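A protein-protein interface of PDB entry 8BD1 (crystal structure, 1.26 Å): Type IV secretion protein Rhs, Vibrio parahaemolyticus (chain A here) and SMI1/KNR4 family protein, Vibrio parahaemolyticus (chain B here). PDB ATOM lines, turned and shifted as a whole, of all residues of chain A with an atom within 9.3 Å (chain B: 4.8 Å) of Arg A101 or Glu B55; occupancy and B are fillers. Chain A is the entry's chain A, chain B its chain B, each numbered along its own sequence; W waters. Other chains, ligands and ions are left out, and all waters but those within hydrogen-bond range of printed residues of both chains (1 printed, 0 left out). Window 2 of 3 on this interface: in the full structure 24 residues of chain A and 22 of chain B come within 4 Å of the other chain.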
ATOM      1  N   LYS A  27     -15.723  26.564  32.057  1.00  0.00           N
ATOM      2  CA  LYS A  27     -15.674  25.593  33.146  1.00  0.00           C
ATOM      3  C   LYS A  27     -14.291  24.965  33.287  1.00  0.00           C
ATOM      4  O   LYS A  27     -13.870  24.638  34.404  1.00  0.00           O
ATOM      5  CB  LYS A  27     -16.751  24.524  32.940  1.00  0.00           C
ATOM      6  CG  LYS A  27     -16.770  23.428  33.991  1.00  0.00           C
ATOM      7  CD  LYS A  27     -17.102  23.988  35.365  1.00  0.00           C
ATOM      8  CE  LYS A  27     -18.504  24.577  35.418  1.00  0.00           C
ATOM      9  NZ  LYS A  27     -18.710  25.371  36.665  1.00  0.00           N
ATOM     10  N   LYS A  76     -14.466   9.963  24.887  1.00  0.00           N
ATOM     11  CA  LYS A  76     -15.446  10.858  24.281  1.00  0.00           C
ATOM     12  C   LYS A  76     -16.274  11.603  25.314  1.00  0.00           C
ATOM     13  O   LYS A  76     -16.910  12.604  24.971  1.00  0.00           O
ATOM     14  CB  LYS A  76     -16.363  10.083  23.334  1.00  0.00           C
ATOM     15  CG  LYS A  76     -15.598   9.275  22.292  1.00  0.00           C
ATOM     16  CD  LYS A  76     -16.452   8.914  21.082  1.00  0.00           C
ATOM     17  CE  LYS A  76     -15.719   9.223  19.775  1.00  0.00           C
ATOM     18  NZ  LYS A  76     -16.481   8.765  18.582  1.00  0.00           N
ATOM     19  N   SER A  77     -16.301  11.139  26.564  1.00  0.00           N
ATOM     20  CA  SER A  77     -16.989  11.908  27.589  1.00  0.00           C
ATOM     21  C   SER A  77     -16.171  13.113  28.029  1.00  0.00           C
ATOM     22  O   SER A  77     -16.728  14.050  28.611  1.00  0.00           O
ATOM     23  CB  SER A  77     -17.346  11.025  28.790  1.00  0.00           C
ATOM     24  OG  SER A  77     -16.215  10.784  29.594  1.00  0.00           O
ATOM     25  N   LYS A  95     -13.738  18.972  26.575  1.00  0.00           N
ATOM     26  CA  LYS A  95     -15.070  19.539  26.377  1.00  0.00           C
ATOM     27  C   LYS A  95     -15.349  20.689  27.330  1.00  0.00           C
ATOM     28  O   LYS A  95     -16.128  21.591  27.001  1.00  0.00           O
ATOM     29  CB  LYS A  95     -16.131  18.461  26.566  1.00  0.00           C
ATOM     30  CG  LYS A  95     -16.125  17.398  25.497  1.00  0.00           C
ATOM     31  CD  LYS A  95     -17.072  16.273  25.882  1.00  0.00           C
ATOM     32  CE  LYS A  95     -17.759  15.677  24.677  1.00  0.00           C
ATOM     33  NZ  LYS A  95     -18.708  14.610  25.099  1.00  0.00           N
ATOM     34  N   SER A  96     -14.728  20.679  28.513  1.00  0.00           N
ATOM     35  CA  SER A  96     -14.978  21.725  29.501  1.00  0.00           C
ATOM     36  C   SER A  96     -14.577  23.113  29.012  1.00  0.00           C
ATOM     37  O   SER A  96     -15.078  24.110  29.551  1.00  0.00           O
ATOM     38  CB  SER A  96     -14.246  21.395  30.799  1.00  0.00           C
ATOM     39  OG  SER A  96     -12.862  21.288  30.552  1.00  0.00           O
ATOM     40  N   VAL A  97     -13.691  23.213  28.022  1.00  0.00           N
ATOM     41  CA  VAL A  97     -13.384  24.497  27.402  1.00  0.00           C
ATOM     42  C   VAL A  97     -13.978  24.642  26.005  1.00  0.00           C
ATOM     43  O   VAL A  97     -14.196  25.780  25.559  1.00  0.00           O
ATOM     44  CB  VAL A  97     -11.871  24.813  27.383  1.00  0.00           C
ATOM     45  CG1 VAL A  97     -11.268  24.680  28.782  1.00  0.00           C
ATOM     46  CG2 VAL A  97     -11.128  23.934  26.403  1.00  0.00           C
ATOM     47  N   HIS A  98     -14.258  23.542  25.313  1.00  0.00           N
ATOM     48  CA  HIS A  98     -14.613  23.569  23.900  1.00  0.00           C
ATOM     49  C   HIS A  98     -16.108  23.536  23.642  1.00  0.00           C
ATOM     50  O   HIS A  98     -16.553  24.052  22.611  1.00  0.00           O
ATOM     51  CB  HIS A  98     -14.002  22.348  23.212  1.00  0.00           C
ATOM     52  CG  HIS A  98     -13.942  22.459  21.721  1.00  0.00           C
ATOM     53  ND1 HIS A  98     -14.923  21.955  20.892  1.00  0.00           N
ATOM     54  CD2 HIS A  98     -13.009  23.009  20.911  1.00  0.00           C
ATOM     55  CE1 HIS A  98     -14.596  22.198  19.636  1.00  0.00           C
ATOM     56  NE2 HIS A  98     -13.439  22.834  19.620  1.00  0.00           N
ATOM     57  N   SER A  99     -16.883  22.921  24.532  1.00  0.00           N
ATOM     58  CA  SER A  99     -18.260  22.528  24.251  1.00  0.00           C
ATOM     59  C   SER A  99     -19.240  23.290  25.129  1.00  0.00           C
ATOM     60  O   SER A  99     -19.186  23.176  26.357  1.00  0.00           O
ATOM     61  CB  SER A  99     -18.461  21.040  24.511  1.00  0.00           C
ATOM     62  OG  SER A  99     -19.725  20.648  24.003  1.00  0.00           O
ATOM     63  N   VAL A 100     -20.186  23.992  24.495  1.00  0.00           N
ATOM     64  CA  VAL A 100     -21.202  24.739  25.240  1.00  0.00           C
ATOM     65  C   VAL A 100     -21.924  23.832  26.228  1.00  0.00           C
ATOM     66  O   VAL A 100     -22.198  24.223  27.369  1.00  0.00           O
ATOM     67  CB  VAL A 100     -22.184  25.422  24.267  1.00  0.00           C
ATOM     68  CG1 VAL A 100     -23.377  26.013  25.025  1.00  0.00           C
ATOM     69  CG2 VAL A 100     -21.474  26.490  23.478  1.00  0.00           C
ATOM     70  N   ARG A 101     -22.227  22.599  25.812  1.00  0.00           N
ATOM     71  CA  ARG A 101     -22.974  21.675  26.658  1.00  0.00           C
ATOM     72  C   ARG A 101     -22.226  21.345  27.945  1.00  0.00           C
ATOM     73  O   ARG A 101     -22.853  20.987  28.953  1.00  0.00           O
ATOM     74  CB  ARG A 101     -23.292  20.400  25.865  1.00  0.00           C
ATOM     75  CG  ARG A 101     -23.999  19.300  26.655  1.00  0.00           C
ATOM     76  CD  ARG A 101     -23.007  18.254  27.150  1.00  0.00           C
ATOM     77  NE  ARG A 101     -23.632  17.179  27.910  1.00  0.00           N
ATOM     78  CZ  ARG A 101     -23.992  17.268  29.186  1.00  0.00           C
ATOM     79  NH1 ARG A 101     -23.827  18.386  29.876  1.00  0.00           N
ATOM     80  NH2 ARG A 101     -24.532  16.208  29.784  1.00  0.00           N
ATOM     81  N   ASN A 102     -20.899  21.453  27.938  1.00  0.00           N
ATOM     82  CA  ASN A 102     -20.069  21.106  29.085  1.00  0.00           C
ATOM     83  C   ASN A 102     -19.486  22.330  29.780  1.00  0.00           C
ATOM     84  O   ASN A 102     -18.545  22.194  30.568  1.00  0.00           O
ATOM     85  CB  ASN A 102     -18.953  20.147  28.669  1.00  0.00           C
ATOM     86  CG  ASN A 102     -19.482  18.902  27.994  1.00  0.00           C
ATOM     87  OD1 ASN A 102     -19.607  18.845  26.774  1.00  0.00           O
ATOM     88  ND2 ASN A 102     -19.804  17.896  28.789  1.00  0.00           N
ATOM     89  N   GLY A 103     -20.013  23.519  29.502  1.00  0.00           N
ATOM     90  CA  GLY A 103     -19.491  24.731  30.104  1.00  0.00           C
ATOM     91  C   GLY A 103     -18.369  25.395  29.338  1.00  0.00           C
ATOM     92  O   GLY A 103     -17.768  26.351  29.851  1.00  0.00           O
ATOM     93  N   GLY A 104     -18.047  24.906  28.136  1.00  0.00           N
ATOM     94  CA  GLY A 104     -17.059  25.530  27.285  1.00  0.00           C
ATOM     95  C   GLY A 104     -17.633  26.736  26.571  1.00  0.00           C
ATOM     96  O   GLY A 104     -18.773  27.138  26.794  1.00  0.00           O
ATOM     97  N   VAL A 105     -16.835  27.312  25.673  1.00  0.00           N
ATOM     98  CA  VAL A 105     -17.192  28.560  25.005  1.00  0.00           C
ATOM     99  C   VAL A 105     -17.567  28.283  23.554  1.00  0.00           C
ATOM    100  O   VAL A 105     -16.819  27.618  22.828  1.00  0.00           O
ATOM    101  CB  VAL A 105     -16.083  29.625  25.122  1.00  0.00           C
ATOM    102  CG1 VAL A 105     -14.740  29.114  24.599  1.00  0.00           C
ATOM    103  CG2 VAL A 105     -16.507  30.916  24.413  1.00  0.00           C
ATOM    104  N   ALA A 106     -18.720  28.809  23.133  1.00  0.00           N
ATOM    105  CA  ALA A 106     -19.134  28.714  21.741  1.00  0.00           C
ATOM    106  C   ALA A 106     -18.153  29.462  20.848  1.00  0.00           C
ATOM    107  O   ALA A 106     -17.654  30.534  21.199  1.00  0.00           O
ATOM    108  CB  ALA A 106     -20.528  29.321  21.568  1.00  0.00           C
ATOM    109  N   GLU B  49     -24.199  11.442  22.505  1.00  0.00           N
ATOM    110  CA  GLU B  49     -24.743  11.571  23.851  1.00  0.00           C
ATOM    111  C   GLU B  49     -26.213  11.947  23.771  1.00  0.00           C
ATOM    112  O   GLU B  49     -26.592  12.815  22.980  1.00  0.00           O
ATOM    113  CB  GLU B  49     -24.014  12.656  24.653  1.00  0.00           C
ATOM    114  CG  GLU B  49     -24.399  12.650  26.131  1.00  0.00           C
ATOM    115  CD  GLU B  49     -23.946  13.871  26.901  1.00  0.00           C
ATOM    116  OE1 GLU B  49     -23.362  14.792  26.306  1.00  0.00           O
ATOM    117  OE2 GLU B  49     -24.190  13.909  28.126  1.00  0.00           O
ATOM    118  N   PHE B  51     -28.689  13.929  25.931  1.00  0.00           N
ATOM    119  CA  PHE B  51     -28.620  14.842  27.072  1.00  0.00           C
ATOM    120  C   PHE B  51     -29.598  14.369  28.145  1.00  0.00           C
ATOM    121  O   PHE B  51     -30.772  14.134  27.846  1.00  0.00           O
ATOM    122  CB  PHE B  51     -28.943  16.275  26.644  1.00  0.00           C
ATOM    123  CG  PHE B  51     -27.924  16.885  25.710  1.00  0.00           C
ATOM    124  CD1 PHE B  51     -26.707  16.263  25.457  1.00  0.00           C
ATOM    125  CD2 PHE B  51     -28.179  18.108  25.101  1.00  0.00           C
ATOM    126  CE1 PHE B  51     -25.780  16.835  24.596  1.00  0.00           C
ATOM    127  CE2 PHE B  51     -27.251  18.680  24.253  1.00  0.00           C
ATOM    128  CZ  PHE B  51     -26.059  18.047  24.001  1.00  0.00           C
ATOM    129  N   PRO B  52     -29.151  14.176  29.382  1.00  0.00           N
ATOM    130  CA  PRO B  52     -30.046  13.651  30.416  1.00  0.00           C
ATOM    131  C   PRO B  52     -31.024  14.696  30.925  1.00  0.00           C
ATOM    132  O   PRO B  52     -30.728  15.893  30.979  1.00  0.00           O
ATOM    133  CB  PRO B  52     -29.095  13.223  31.542  1.00  0.00           C
ATOM    134  CG  PRO B  52     -27.770  13.821  31.241  1.00  0.00           C
ATOM    135  CD  PRO B  52     -27.791  14.448  29.873  1.00  0.00           C
ATOM    136  N   LYS B  53     -32.198  14.203  31.328  1.00  0.00           N
ATOM    137  CA  LYS B  53     -33.244  15.071  31.861  1.00  0.00           C
ATOM    138  C   LYS B  53     -32.740  15.930  33.014  1.00  0.00           C
ATOM    139  O   LYS B  53     -33.044  17.128  33.085  1.00  0.00           O
ATOM    140  CB  LYS B  53     -34.444  14.227  32.300  1.00  0.00           C
ATOM    141  CG  LYS B  53     -35.622  15.057  32.808  1.00  0.00           C
ATOM    142  CD  LYS B  53     -36.596  14.226  33.627  1.00  0.00           C
ATOM    143  CE  LYS B  53     -37.369  13.260  32.747  1.00  0.00           C
ATOM    144  NZ  LYS B  53     -38.757  13.028  33.255  1.00  0.00           N
ATOM    145  N   ASP B  54     -31.955  15.347  33.918  1.00  0.00           N
ATOM    146  CA  ASP B  54     -31.542  16.108  35.093  1.00  0.00           C
ATOM    147  C   ASP B  54     -30.490  17.168  34.791  1.00  0.00           C
ATOM    148  O   ASP B  54     -30.075  17.885  35.705  1.00  0.00           O
ATOM    149  CB  ASP B  54     -31.116  15.187  36.245  1.00  0.00           C
ATOM    150  CG  ASP B  54     -29.897  14.340  35.921  1.00  0.00           C
ATOM    151  OD1 ASP B  54     -29.305  14.486  34.833  1.00  0.00           O
ATOM    152  OD2 ASP B  54     -29.528  13.505  36.773  1.00  0.00           O
ATOM    153  N   GLU B  55     -30.061  17.299  33.536  1.00  0.00           N
ATOM    154  CA  GLU B  55     -29.122  18.337  33.154  1.00  0.00           C
ATOM    155  C   GLU B  55     -29.696  19.350  32.176  1.00  0.00           C
ATOM    156  O   GLU B  55     -28.986  20.289  31.811  1.00  0.00           O
ATOM    157  CB  GLU B  55     -27.856  17.716  32.551  1.00  0.00           C
ATOM    158  CG  GLU B  55     -26.953  17.045  33.561  1.00  0.00           C
ATOM    159  CD  GLU B  55     -25.617  16.684  32.961  1.00  0.00           C
ATOM    160  OE1 GLU B  55     -24.843  17.608  32.635  1.00  0.00           O
ATOM    161  OE2 GLU B  55     -25.350  15.477  32.802  1.00  0.00           O
ATOM    162  N   LEU B  56     -30.948  19.194  31.740  1.00  0.00           N
ATOM    163  CA  LEU B  56     -31.467  20.078  30.699  1.00  0.00           C
ATOM    164  C   LEU B  56     -31.465  21.534  31.141  1.00  0.00           C
ATOM    165  O   LEU B  56     -31.179  22.430  30.339  1.00  0.00           O
ATOM    166  CB  LEU B  56     -32.869  19.650  30.280  1.00  0.00           C
ATOM    167  CG  LEU B  56     -33.011  18.306  29.568  1.00  0.00           C
ATOM    168  CD1 LEU B  56     -34.407  18.149  28.981  1.00  0.00           C
ATOM    169  CD2 LEU B  56     -31.944  18.130  28.495  1.00  0.00           C
ATOM    170  N   GLU B  57     -31.779  21.799  32.411  1.00  0.00           N
ATOM    171  CA  GLU B  57     -31.817  23.184  32.868  1.00  0.00           C
ATOM    172  C   GLU B  57     -30.448  23.836  32.754  1.00  0.00           C
ATOM    173  O   GLU B  57     -30.322  24.952  32.240  1.00  0.00           O
ATOM    174  CB  GLU B  57     -32.351  23.278  34.298  1.00  0.00           C
ATOM    175  CG  GLU B  57     -32.573  24.715  34.743  1.00  0.00           C
ATOM    176  CD  GLU B  57     -33.315  24.829  36.062  1.00  0.00           C
ATOM    177  OE1 GLU B  57     -33.555  23.791  36.714  1.00  0.00           O
ATOM    178  OE2 GLU B  57     -33.655  25.967  36.448  1.00  0.00           O
ATOM    179  N   ASP B  58     -29.402  23.143  33.210  1.00  0.00           N
ATOM    180  CA  ASP B  58     -28.054  23.688  33.103  1.00  0.00           C
ATOM    181  C   ASP B  58     -27.612  23.790  31.649  1.00  0.00           C
ATOM    182  O   ASP B  58     -26.948  24.758  31.265  1.00  0.00           O
ATOM    183  CB  ASP B  58     -27.070  22.819  33.884  1.00  0.00           C
ATOM    184  CG  ASP B  58     -25.628  23.246  33.677  1.00  0.00           C
ATOM    185  OD1 ASP B  58     -25.257  24.347  34.141  1.00  0.00           O
ATOM    186  OD2 ASP B  58     -24.864  22.490  33.035  1.00  0.00           O
ATOM    187  N   ILE B  59     -27.957  22.792  30.832  1.00  0.00           N
ATOM    188  CA  ILE B  59     -27.577  22.837  29.421  1.00  0.00           C
ATOM    189  C   ILE B  59     -28.256  24.012  28.728  1.00  0.00           C
ATOM    190  O   ILE B  59     -27.619  24.761  27.978  1.00  0.00           O
ATOM    191  CB  ILE B  59     -27.876  21.493  28.731  1.00  0.00           C
ATOM    192  CG1 ILE B  59     -26.992  20.389  29.318  1.00  0.00           C
ATOM    193  CG2 ILE B  59     -27.644  21.604  27.229  1.00  0.00           C
ATOM    194  CD1 ILE B  59     -27.378  19.001  28.860  1.00  0.00           C
ATOM    195  N   ASN B  62     -26.766  27.339  29.294  1.00  0.00           N
ATOM    196  CA  ASN B  62     -25.600  27.606  28.461  1.00  0.00           C
ATOM    197  C   ASN B  62     -25.950  27.835  26.997  1.00  0.00           C
ATOM    198  O   ASN B  62     -25.270  28.617  26.323  1.00  0.00           O
ATOM    199  CB  ASN B  62     -24.595  26.459  28.575  1.00  0.00           C
ATOM    200  CG  ASN B  62     -23.900  26.438  29.915  1.00  0.00           C
ATOM    201  OD1 ASN B  62     -23.677  27.491  30.516  1.00  0.00           O
ATOM    202  ND2 ASN B  62     -23.540  25.252  30.381  1.00  0.00           N
ATOM    203  N   TYR B  63     -26.997  27.192  26.495  1.00  0.00           N
ATOM    204  CA  TYR B  63     -27.339  27.283  25.082  1.00  0.00           C
ATOM    205  C   TYR B  63     -28.365  28.362  24.758  1.00  0.00           C
ATOM    206  O   TYR B  63     -28.481  28.742  23.585  1.00  0.00           O
ATOM    207  CB  TYR B  63     -27.893  25.944  24.584  1.00  0.00           C
ATOM    208  CG  TYR B  63     -26.871  25.164  23.797  1.00  0.00           C
ATOM    209  CD1 TYR B  63     -26.456  25.622  22.561  1.00  0.00           C
ATOM    210  CD2 TYR B  63     -26.323  23.974  24.278  1.00  0.00           C
ATOM    211  CE1 TYR B  63     -25.519  24.945  21.816  1.00  0.00           C
ATOM    212  CE2 TYR B  63     -25.373  23.278  23.524  1.00  0.00           C
ATOM    213  CZ  TYR B  63     -24.984  23.783  22.301  1.00  0.00           C
ATOM    214  OH  TYR B  63     -24.050  23.135  21.525  1.00  0.00           O
HETATM  215  O   HOH W   1     -22.223  21.424  23.004  1.00  0.00           O
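Among the printed residues, pairs that only touch across the chains: Arg A101 with Phe B51 (3.6 Å), Val A100 with Tyr B63 (3.7 Å), Arg A101 with Pro B52 (3.7 Å), Arg A101 with Ile B59 (3.7 Å) and Arg A101 with Tyr B63 (3.9 Å).
NH2 of Arg A101 is in salt-bridge range of OE2 of Glu B49, at 2.9 Å.
O of Val A100 is in hydrogen-bond range of ND2 of Asn B62, at 3.5 Å.
NH1 of Arg A101 lies within salt-bridge range of OE1 of Glu B55 (3.0 Å).
Val A97 touches none of the printed residues of chain B.
Arg A101 touches just these residues of chain B: Glu B49, Phe B51, Pro B52, Glu B55, Ile B59 and Tyr B63.
Of the printed residues of chain A, Phe B51 touches Arg A101 (3.6 Å).
Of chain A, only Arg A101 comes within 4 Å of Pro B52.
Asp B54 touches none of the printed residues of chain A.
Of chain A, only Arg A101 (3.0 Å) comes within 4 Å of Glu B55.
Of the printed residues of chain A, Asn B62 touches Val A100 (3.5 Å).
Of the 12 printed residues of chain B, 7 touch a printed residue of chain A.
Printed residues of chain B that touch a printed residue of chain A: Glu B49, Phe B51, Pro B52, Glu B55, Ile B59, Asn B62 and Tyr B63.
Hydrophobic or aromatic side chains of chain B within 4 Å of the printed part of chain A: Phe B51, Pro B52, Ile B59 and Tyr B63.
Of the 15 printed residues of chain A, 2 touch a printed residue of chain B.
Among the printed residues, 8 pairs touch across the chains.
Water W1 lies within hydrogen-bond range of the side-chain hydroxyl (OG) of Ser A99, the side-chain hydroxyl (OH) of Tyr B63 and the backbone NH (N) of Arg A101.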
